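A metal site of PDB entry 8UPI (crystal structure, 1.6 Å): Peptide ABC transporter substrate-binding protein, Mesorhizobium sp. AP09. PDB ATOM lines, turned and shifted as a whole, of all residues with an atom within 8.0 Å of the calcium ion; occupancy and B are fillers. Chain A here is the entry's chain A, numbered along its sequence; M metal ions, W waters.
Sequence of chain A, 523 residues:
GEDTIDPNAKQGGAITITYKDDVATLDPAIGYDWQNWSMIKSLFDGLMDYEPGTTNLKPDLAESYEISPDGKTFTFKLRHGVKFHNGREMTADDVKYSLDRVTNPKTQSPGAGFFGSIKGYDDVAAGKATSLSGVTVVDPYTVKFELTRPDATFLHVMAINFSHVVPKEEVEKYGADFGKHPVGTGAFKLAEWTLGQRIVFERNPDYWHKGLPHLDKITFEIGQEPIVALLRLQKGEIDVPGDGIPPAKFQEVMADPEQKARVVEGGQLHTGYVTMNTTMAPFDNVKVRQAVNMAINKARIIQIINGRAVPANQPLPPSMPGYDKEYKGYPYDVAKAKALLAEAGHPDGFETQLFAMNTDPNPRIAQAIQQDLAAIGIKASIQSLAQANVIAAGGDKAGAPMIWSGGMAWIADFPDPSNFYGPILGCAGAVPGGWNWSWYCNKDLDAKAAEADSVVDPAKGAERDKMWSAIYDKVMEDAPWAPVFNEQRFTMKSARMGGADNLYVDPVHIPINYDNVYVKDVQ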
ATOM      1  N   SER A  38      15.675  24.386  13.920  1.00  0.00           N
ATOM      2  CA  SER A  38      16.541  25.410  14.492  1.00  0.00           C
ATOM      3  C   SER A  38      17.804  24.803  15.102  1.00  0.00           C
ATOM      4  O   SER A  38      18.846  25.476  15.151  1.00  0.00           O
ATOM      5  CB  SER A  38      15.790  26.235  15.535  1.00  0.00           C
ATOM      6  OG  SER A  38      16.510  27.409  15.868  1.00  0.00           O
ATOM      7  N   MET A  39      17.733  23.565  15.580  1.00  0.00           N
ATOM      8  CA  MET A  39      18.946  22.849  15.975  1.00  0.00           C
ATOM      9  C   MET A  39      19.954  22.846  14.838  1.00  0.00           C
ATOM     10  O   MET A  39      21.135  23.186  15.017  1.00  0.00           O
ATOM     11  CB  MET A  39      18.623  21.409  16.369  1.00  0.00           C
ATOM     12  CG  MET A  39      17.755  21.232  17.593  1.00  0.00           C
ATOM     13  SD  MET A  39      17.477  19.464  17.880  1.00  0.00           S
ATOM     14  CE  MET A  39      16.320  19.539  19.234  1.00  0.00           C
ATOM     15  N   ILE A  40      19.506  22.437  13.656  1.00  0.00           N
ATOM     16  CA  ILE A  40      20.385  22.359  12.499  1.00  0.00           C
ATOM     17  C   ILE A  40      20.942  23.738  12.146  1.00  0.00           C
ATOM     18  O   ILE A  40      22.127  23.879  11.834  1.00  0.00           O
ATOM     19  CB  ILE A  40      19.619  21.702  11.332  1.00  0.00           C
ATOM     20  CG1 ILE A  40      19.360  20.233  11.684  1.00  0.00           C
ATOM     21  CG2 ILE A  40      20.379  21.846   9.979  1.00  0.00           C
ATOM     22  CD1 ILE A  40      18.349  19.517  10.780  1.00  0.00           C
ATOM     23  N   LYS A  41      20.110  24.787  12.240  1.00  0.00           N
ATOM     24  CA  LYS A  41      20.611  26.140  11.947  1.00  0.00           C
ATOM     25  C   LYS A  41      21.699  26.570  12.914  1.00  0.00           C
ATOM     26  O   LYS A  41      22.507  27.446  12.569  1.00  0.00           O
ATOM     27  CB  LYS A  41      19.488  27.172  11.977  1.00  0.00           C
ATOM     28  CG  LYS A  41      18.534  27.127  10.786  1.00  0.00           C
ATOM     29  CD  LYS A  41      17.543  28.307  10.821  1.00  0.00           C
ATOM     30  CE  LYS A  41      16.587  28.285   9.621  1.00  0.00           C
ATOM     31  NZ  LYS A  41      17.313  28.485   8.352  1.00  0.00           N
ATOM     32  N   SER A  42      21.756  25.991  14.105  1.00  0.00           N
ATOM     33  CA  SER A  42      22.809  26.344  15.039  1.00  0.00           C
ATOM     34  C   SER A  42      24.083  25.529  14.845  1.00  0.00           C
ATOM     35  O   SER A  42      25.166  25.993  15.244  1.00  0.00           O
ATOM     36  CB  SER A  42      22.296  26.213  16.477  1.00  0.00           C
ATOM     37  OG  SER A  42      21.460  27.326  16.795  1.00  0.00           O
ATOM     38  N   LEU A  43      24.003  24.357  14.236  1.00  0.00           N
ATOM     39  CA  LEU A  43      25.193  23.568  13.946  1.00  0.00           C
ATOM     40  C   LEU A  43      25.831  23.918  12.607  1.00  0.00           C
ATOM     41  O   LEU A  43      27.032  23.698  12.436  1.00  0.00           O
ATOM     42  CB  LEU A  43      24.840  22.067  13.928  1.00  0.00           C
ATOM     43  CG  LEU A  43      24.380  21.416  15.238  1.00  0.00           C
ATOM     44  CD1 LEU A  43      24.027  19.956  14.951  1.00  0.00           C
ATOM     45  CD2 LEU A  43      25.437  21.506  16.328  1.00  0.00           C
ATOM     46  N   PHE A  44      25.061  24.500  11.684  1.00  0.00           N
ATOM     47  CA  PHE A  44      25.516  24.766  10.334  1.00  0.00           C
ATOM     48  C   PHE A  44      25.238  26.221   9.965  1.00  0.00           C
ATOM     49  O   PHE A  44      24.519  26.936  10.670  1.00  0.00           O
ATOM     50  CB  PHE A  44      24.832  23.833   9.321  1.00  0.00           C
ATOM     51  CG  PHE A  44      25.139  22.371   9.529  1.00  0.00           C
ATOM     52  CD1 PHE A  44      24.364  21.611  10.370  1.00  0.00           C
ATOM     53  CD2 PHE A  44      26.191  21.781   8.862  1.00  0.00           C
ATOM     54  CE1 PHE A  44      24.641  20.260  10.575  1.00  0.00           C
ATOM     55  CE2 PHE A  44      26.476  20.436   9.046  1.00  0.00           C
ATOM     56  CZ  PHE A  44      25.692  19.670   9.908  1.00  0.00           C
ATOM     57  N   ASP A  45      25.793  26.649   8.822  1.00  0.00           N
ATOM     58  CA  ASP A  45      25.529  27.963   8.244  1.00  0.00           C
ATOM     59  C   ASP A  45      25.429  27.852   6.729  1.00  0.00           C
ATOM     60  O   ASP A  45      26.028  26.966   6.128  1.00  0.00           O
ATOM     61  CB  ASP A  45      26.641  28.986   8.550  1.00  0.00           C
ATOM     62  CG  ASP A  45      26.950  29.096  10.031  1.00  0.00           C
ATOM     63  OD1 ASP A  45      26.089  29.620  10.760  1.00  0.00           O
ATOM     64  OD2 ASP A  45      28.055  28.699  10.444  1.00  0.00           O
ATOM     65  N   GLY A  46      24.677  28.773   6.123  1.00  0.00           N
ATOM     66  CA  GLY A  46      24.680  28.940   4.680  1.00  0.00           C
ATOM     67  C   GLY A  46      25.201  30.301   4.276  1.00  0.00           C
ATOM     68  O   GLY A  46      25.711  31.060   5.114  1.00  0.00           O
ATOM     69  N   MET A  48      23.589  32.951   3.450  1.00  0.00           N
ATOM     70  CA  MET A  48      22.770  34.012   4.005  1.00  0.00           C
ATOM     71  C   MET A  48      22.167  33.545   5.318  1.00  0.00           C
ATOM     72  O   MET A  48      22.031  32.340   5.590  1.00  0.00           O
ATOM     73  CB  MET A  48      21.660  34.384   3.030  1.00  0.00           C
ATOM     74  CG  MET A  48      22.165  34.958   1.705  1.00  0.00           C
ATOM     75  SD  MET A  48      23.029  36.539   1.745  1.00  0.00           S
ATOM     76  CE  MET A  48      21.700  37.639   2.245  1.00  0.00           C
ATOM     77  N   ASP A  49      21.796  34.516   6.148  1.00  0.00           N
ATOM     78  CA  ASP A  49      21.015  34.252   7.356  1.00  0.00           C
ATOM     79  C   ASP A  49      20.114  35.476   7.541  1.00  0.00           C
ATOM     80  O   ASP A  49      19.813  36.188   6.573  1.00  0.00           O
ATOM     81  CB  ASP A  49      21.930  33.970   8.561  1.00  0.00           C
ATOM     82  CG  ASP A  49      21.216  33.261   9.714  1.00  0.00           C
ATOM     83  OD1 ASP A  49      19.982  33.067   9.684  1.00  0.00           O
ATOM     84  OD2 ASP A  49      21.914  32.936  10.692  1.00  0.00           O
ATOM     85  N   ASP A  60      25.888  35.775   5.673  1.00  0.00           N
ATOM     86  CA  ASP A  60      26.384  34.927   6.749  1.00  0.00           C
ATOM     87  C   ASP A  60      27.751  34.391   6.337  1.00  0.00           C
ATOM     88  O   ASP A  60      28.764  35.072   6.538  1.00  0.00           O
ATOM     89  CB  ASP A  60      25.358  33.812   7.017  1.00  0.00           C
ATOM     90  CG  ASP A  60      25.398  33.300   8.432  1.00  0.00           C
ATOM     91  OD1 ASP A  60      25.524  34.116   9.382  1.00  0.00           O
ATOM     92  OD2 ASP A  60      25.244  32.067   8.613  1.00  0.00           O
ATOM     93  N   LEU A  61      27.805  33.208   5.694  1.00  0.00           N
ATOM     94  CA  LEU A  61      29.090  32.734   5.188  1.00  0.00           C
ATOM     95  C   LEU A  61      29.588  33.572   4.027  1.00  0.00           C
ATOM     96  O   LEU A  61      30.791  33.605   3.759  1.00  0.00           O
ATOM     97  CB  LEU A  61      28.985  31.268   4.754  1.00  0.00           C
ATOM     98  CG  LEU A  61      28.844  30.259   5.898  1.00  0.00           C
ATOM     99  CD1 LEU A  61      28.775  28.872   5.287  1.00  0.00           C
ATOM    100  CD2 LEU A  61      29.986  30.381   6.908  1.00  0.00           C
ATOM    101  N   ALA A 159      19.531  31.159   2.405  1.00  0.00           N
ATOM    102  CA  ALA A 159      19.510  31.121   3.856  1.00  0.00           C
ATOM    103  C   ALA A 159      18.822  29.883   4.430  1.00  0.00           C
ATOM    104  O   ALA A 159      18.885  29.665   5.649  1.00  0.00           O
ATOM    105  CB  ALA A 159      18.806  32.380   4.399  1.00  0.00           C
ATOM    106  N   ASN A 161      17.962  25.912   5.339  1.00  0.00           N
ATOM    107  CA  ASN A 161      18.856  24.851   5.813  1.00  0.00           C
ATOM    108  C   ASN A 161      19.447  24.042   4.676  1.00  0.00           C
ATOM    109  O   ASN A 161      20.582  23.557   4.763  1.00  0.00           O
ATOM    110  CB  ASN A 161      18.119  23.887   6.743  1.00  0.00           C
ATOM    111  CG  ASN A 161      17.785  24.496   8.095  1.00  0.00           C
ATOM    112  OD1 ASN A 161      17.646  25.709   8.231  1.00  0.00           O
ATOM    113  ND2 ASN A 161      17.620  23.646   9.087  1.00  0.00           N
ATOM    114  N   HIS A 164      22.702  25.092   3.548  1.00  0.00           N
ATOM    115  CA  HIS A 164      23.793  25.163   4.527  1.00  0.00           C
ATOM    116  C   HIS A 164      24.954  24.250   4.091  1.00  0.00           C
ATOM    117  O   HIS A 164      24.758  23.273   3.365  1.00  0.00           O
ATOM    118  CB  HIS A 164      23.291  24.761   5.921  1.00  0.00           C
ATOM    119  CG  HIS A 164      22.496  25.840   6.617  1.00  0.00           C
ATOM    120  ND1 HIS A 164      21.879  26.868   5.944  1.00  0.00           N
ATOM    121  CD2 HIS A 164      22.236  26.029   7.935  1.00  0.00           C
ATOM    122  CE1 HIS A 164      21.265  27.658   6.820  1.00  0.00           C
ATOM    123  NE2 HIS A 164      21.461  27.159   8.032  1.00  0.00           N
ATOM    124  N   THR A 185      29.831  24.490  10.245  1.00  0.00           N
ATOM    125  CA  THR A 185      30.567  25.696  10.589  1.00  0.00           C
ATOM    126  C   THR A 185      29.905  26.488  11.708  1.00  0.00           C
ATOM    127  O   THR A 185      30.415  27.546  12.080  1.00  0.00           O
ATOM    128  CB  THR A 185      30.745  26.605   9.360  1.00  0.00           C
ATOM    129  OG1 THR A 185      29.462  27.029   8.872  1.00  0.00           O
ATOM    130  CG2 THR A 185      31.483  25.882   8.233  1.00  0.00           C
ATOM    131  N   GLY A 186      28.810  25.976  12.269  1.00  0.00           N
ATOM    132  CA  GLY A 186      27.903  26.772  13.053  1.00  0.00           C
ATOM    133  C   GLY A 186      28.393  27.087  14.450  1.00  0.00           C
ATOM    134  O   GLY A 186      29.449  26.636  14.892  1.00  0.00           O
ATOM    135  N   ALA A 187      27.584  27.877  15.141  1.00  0.00           N
ATOM    136  CA  ALA A 187      27.929  28.439  16.444  1.00  0.00           C
ATOM    137  C   ALA A 187      28.028  27.377  17.539  1.00  0.00           C
ATOM    138  O   ALA A 187      28.714  27.602  18.545  1.00  0.00           O
ATOM    139  CB  ALA A 187      26.897  29.489  16.833  1.00  0.00           C
ATOM    140  N   PHE A 188      27.344  26.259  17.388  1.00  0.00           N
ATOM    141  CA  PHE A 188      27.452  25.145  18.309  1.00  0.00           C
ATOM    142  C   PHE A 188      27.965  23.915  17.562  1.00  0.00           C
ATOM    143  O   PHE A 188      27.787  23.796  16.349  1.00  0.00           O
ATOM    144  CB  PHE A 188      26.100  24.811  18.966  1.00  0.00           C
ATOM    145  CG  PHE A 188      25.594  25.871  19.894  1.00  0.00           C
ATOM    146  CD1 PHE A 188      24.796  26.908  19.416  1.00  0.00           C
ATOM    147  CD2 PHE A 188      25.881  25.824  21.247  1.00  0.00           C
ATOM    148  CE1 PHE A 188      24.316  27.884  20.259  1.00  0.00           C
ATOM    149  CE2 PHE A 188      25.411  26.804  22.110  1.00  0.00           C
ATOM    150  CZ  PHE A 188      24.617  27.833  21.622  1.00  0.00           C
ATOM    151  N   TYR A 207      33.959  29.624  16.157  1.00  0.00           N
ATOM    152  CA  TYR A 207      32.930  30.133  15.257  1.00  0.00           C
ATOM    153  C   TYR A 207      33.388  31.426  14.601  1.00  0.00           C
ATOM    154  O   TYR A 207      33.914  32.336  15.256  1.00  0.00           O
ATOM    155  CB  TYR A 207      31.633  30.372  16.032  1.00  0.00           C
ATOM    156  CG  TYR A 207      30.429  30.647  15.154  1.00  0.00           C
ATOM    157  CD1 TYR A 207      30.207  29.916  14.000  1.00  0.00           C
ATOM    158  CD2 TYR A 207      29.500  31.622  15.507  1.00  0.00           C
ATOM    159  CE1 TYR A 207      29.078  30.161  13.199  1.00  0.00           C
ATOM    160  CE2 TYR A 207      28.385  31.863  14.726  1.00  0.00           C
ATOM    161  CZ  TYR A 207      28.181  31.142  13.572  1.00  0.00           C
ATOM    162  OH  TYR A 207      27.070  31.396  12.790  1.00  0.00           O
ATOM    163  N   TRP A 208      33.147  31.533  13.290  1.00  0.00           N
ATOM    164  CA  TRP A 208      33.645  32.681  12.546  1.00  0.00           C
ATOM    165  C   TRP A 208      32.974  33.965  12.999  1.00  0.00           C
ATOM    166  O   TRP A 208      33.557  35.041  12.880  1.00  0.00           O
ATOM    167  CB  TRP A 208      33.424  32.462  11.048  1.00  0.00           C
ATOM    168  CG  TRP A 208      31.994  32.230  10.710  1.00  0.00           C
ATOM    169  CD1 TRP A 208      31.343  31.035  10.614  1.00  0.00           C
ATOM    170  CD2 TRP A 208      31.023  33.243  10.445  1.00  0.00           C
ATOM    171  NE1 TRP A 208      30.025  31.240  10.307  1.00  0.00           N
ATOM    172  CE2 TRP A 208      29.796  32.590  10.201  1.00  0.00           C
ATOM    173  CE3 TRP A 208      31.069  34.636  10.396  1.00  0.00           C
ATOM    174  CZ2 TRP A 208      28.640  33.287   9.885  1.00  0.00           C
ATOM    175  CZ3 TRP A 208      29.905  35.329  10.089  1.00  0.00           C
ATOM    176  CH2 TRP A 208      28.715  34.651   9.843  1.00  0.00           C
ATOM    177  N   HIS A 509      14.658  31.191  12.842  1.00  0.00           N
ATOM    178  CA  HIS A 509      15.212  30.169  13.718  1.00  0.00           C
ATOM    179  C   HIS A 509      14.080  29.716  14.644  1.00  0.00           C
ATOM    180  O   HIS A 509      14.051  30.027  15.842  1.00  0.00           O
ATOM    181  CB  HIS A 509      16.427  30.701  14.457  1.00  0.00           C
ATOM    182  CG  HIS A 509      17.561  31.073  13.547  1.00  0.00           C
ATOM    183  ND1 HIS A 509      18.740  30.378  13.502  1.00  0.00           N
ATOM    184  CD2 HIS A 509      17.659  32.054  12.613  1.00  0.00           C
ATOM    185  CE1 HIS A 509      19.539  30.923  12.599  1.00  0.00           C
ATOM    186  NE2 HIS A 509      18.907  31.936  12.036  1.00  0.00           N
ATOM    187  N   ASP A 515      21.597  30.876  18.957  1.00  0.00           N
ATOM    188  CA  ASP A 515      22.883  31.551  18.870  1.00  0.00           C
ATOM    189  C   ASP A 515      22.903  32.903  19.560  1.00  0.00           C
ATOM    190  O   ASP A 515      23.982  33.393  19.900  1.00  0.00           O
ATOM    191  CB  ASP A 515      23.299  31.766  17.409  1.00  0.00           C
ATOM    192  CG  ASP A 515      23.503  30.470  16.646  1.00  0.00           C
ATOM    193  OD1 ASP A 515      23.370  29.373  17.244  1.00  0.00           O
ATOM    194  OD2 ASP A 515      23.798  30.573  15.432  1.00  0.00           O
HETATM  195 CA    CA M   1      23.923  29.009  11.653  1.00  0.00          CA
HETATM  196  O   HOH W   1      24.001  31.375  10.921  1.00  0.00           O
HETATM  197  O   HOH W   2      22.342  29.203   9.868  1.00  0.00           O
HETATM  198  O   HOH W   3      22.545  30.416  13.081  1.00  0.00           O
HETATM  199  O   HOH W   4      25.116  28.896  13.862  1.00  0.00           O
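NZ of Lys 41 sits at hydrogen-bond distance from O of Ala 159, 3.3 Å away. NZ of Lys 41 is in hydrogen-bond range of OD1 of Asn 161 (2.8 Å). OH of Tyr 207 sits close to OD1 of Asp 45, 2.9 Å away. The side-chain carboxylate of Asp 45 sits close to the backbone NH of Gly 186 (3.4 Å). The side-chain hydroxyl of Thr 185 sits at hydrogen-bond distance from the side-chain carboxylate of Asp 45 (2.7 Å). The side-chain carboxylate (OD2) of Asp 45 is in hydrogen-bond range of the indole nitrogen (NE1) of Trp 208 (3.2 Å).
O of Lys 41 is bound to the calcium ion (2.3 Å). O of Phe 44 binds the calcium ion. Water W2 binds the calcium ion, at 2.4 Å. The calcium ion is bound by the side-chain carboxylate (OD1) of Asp 45, 2.4 Å away. The calcium ion is bound by water W3, at 2.4 Å. Water W1 is bound to the calcium ion (2.5 Å). Water W4 binds the calcium ion, at 2.5 Å. The calcium ion has seven donor atoms within binding distance.
Water W4 lies within hydrogen-bond range of OD2 of Asp 515 (2.6 Å), N of Ala 187 (3.0 Å), O of Ser 42 (3.2 Å) and OH of Tyr 207 (3.3 Å). Water W1 lies within hydrogen-bond range of OD2 of Asp 49 and OD2 of Asp 60.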
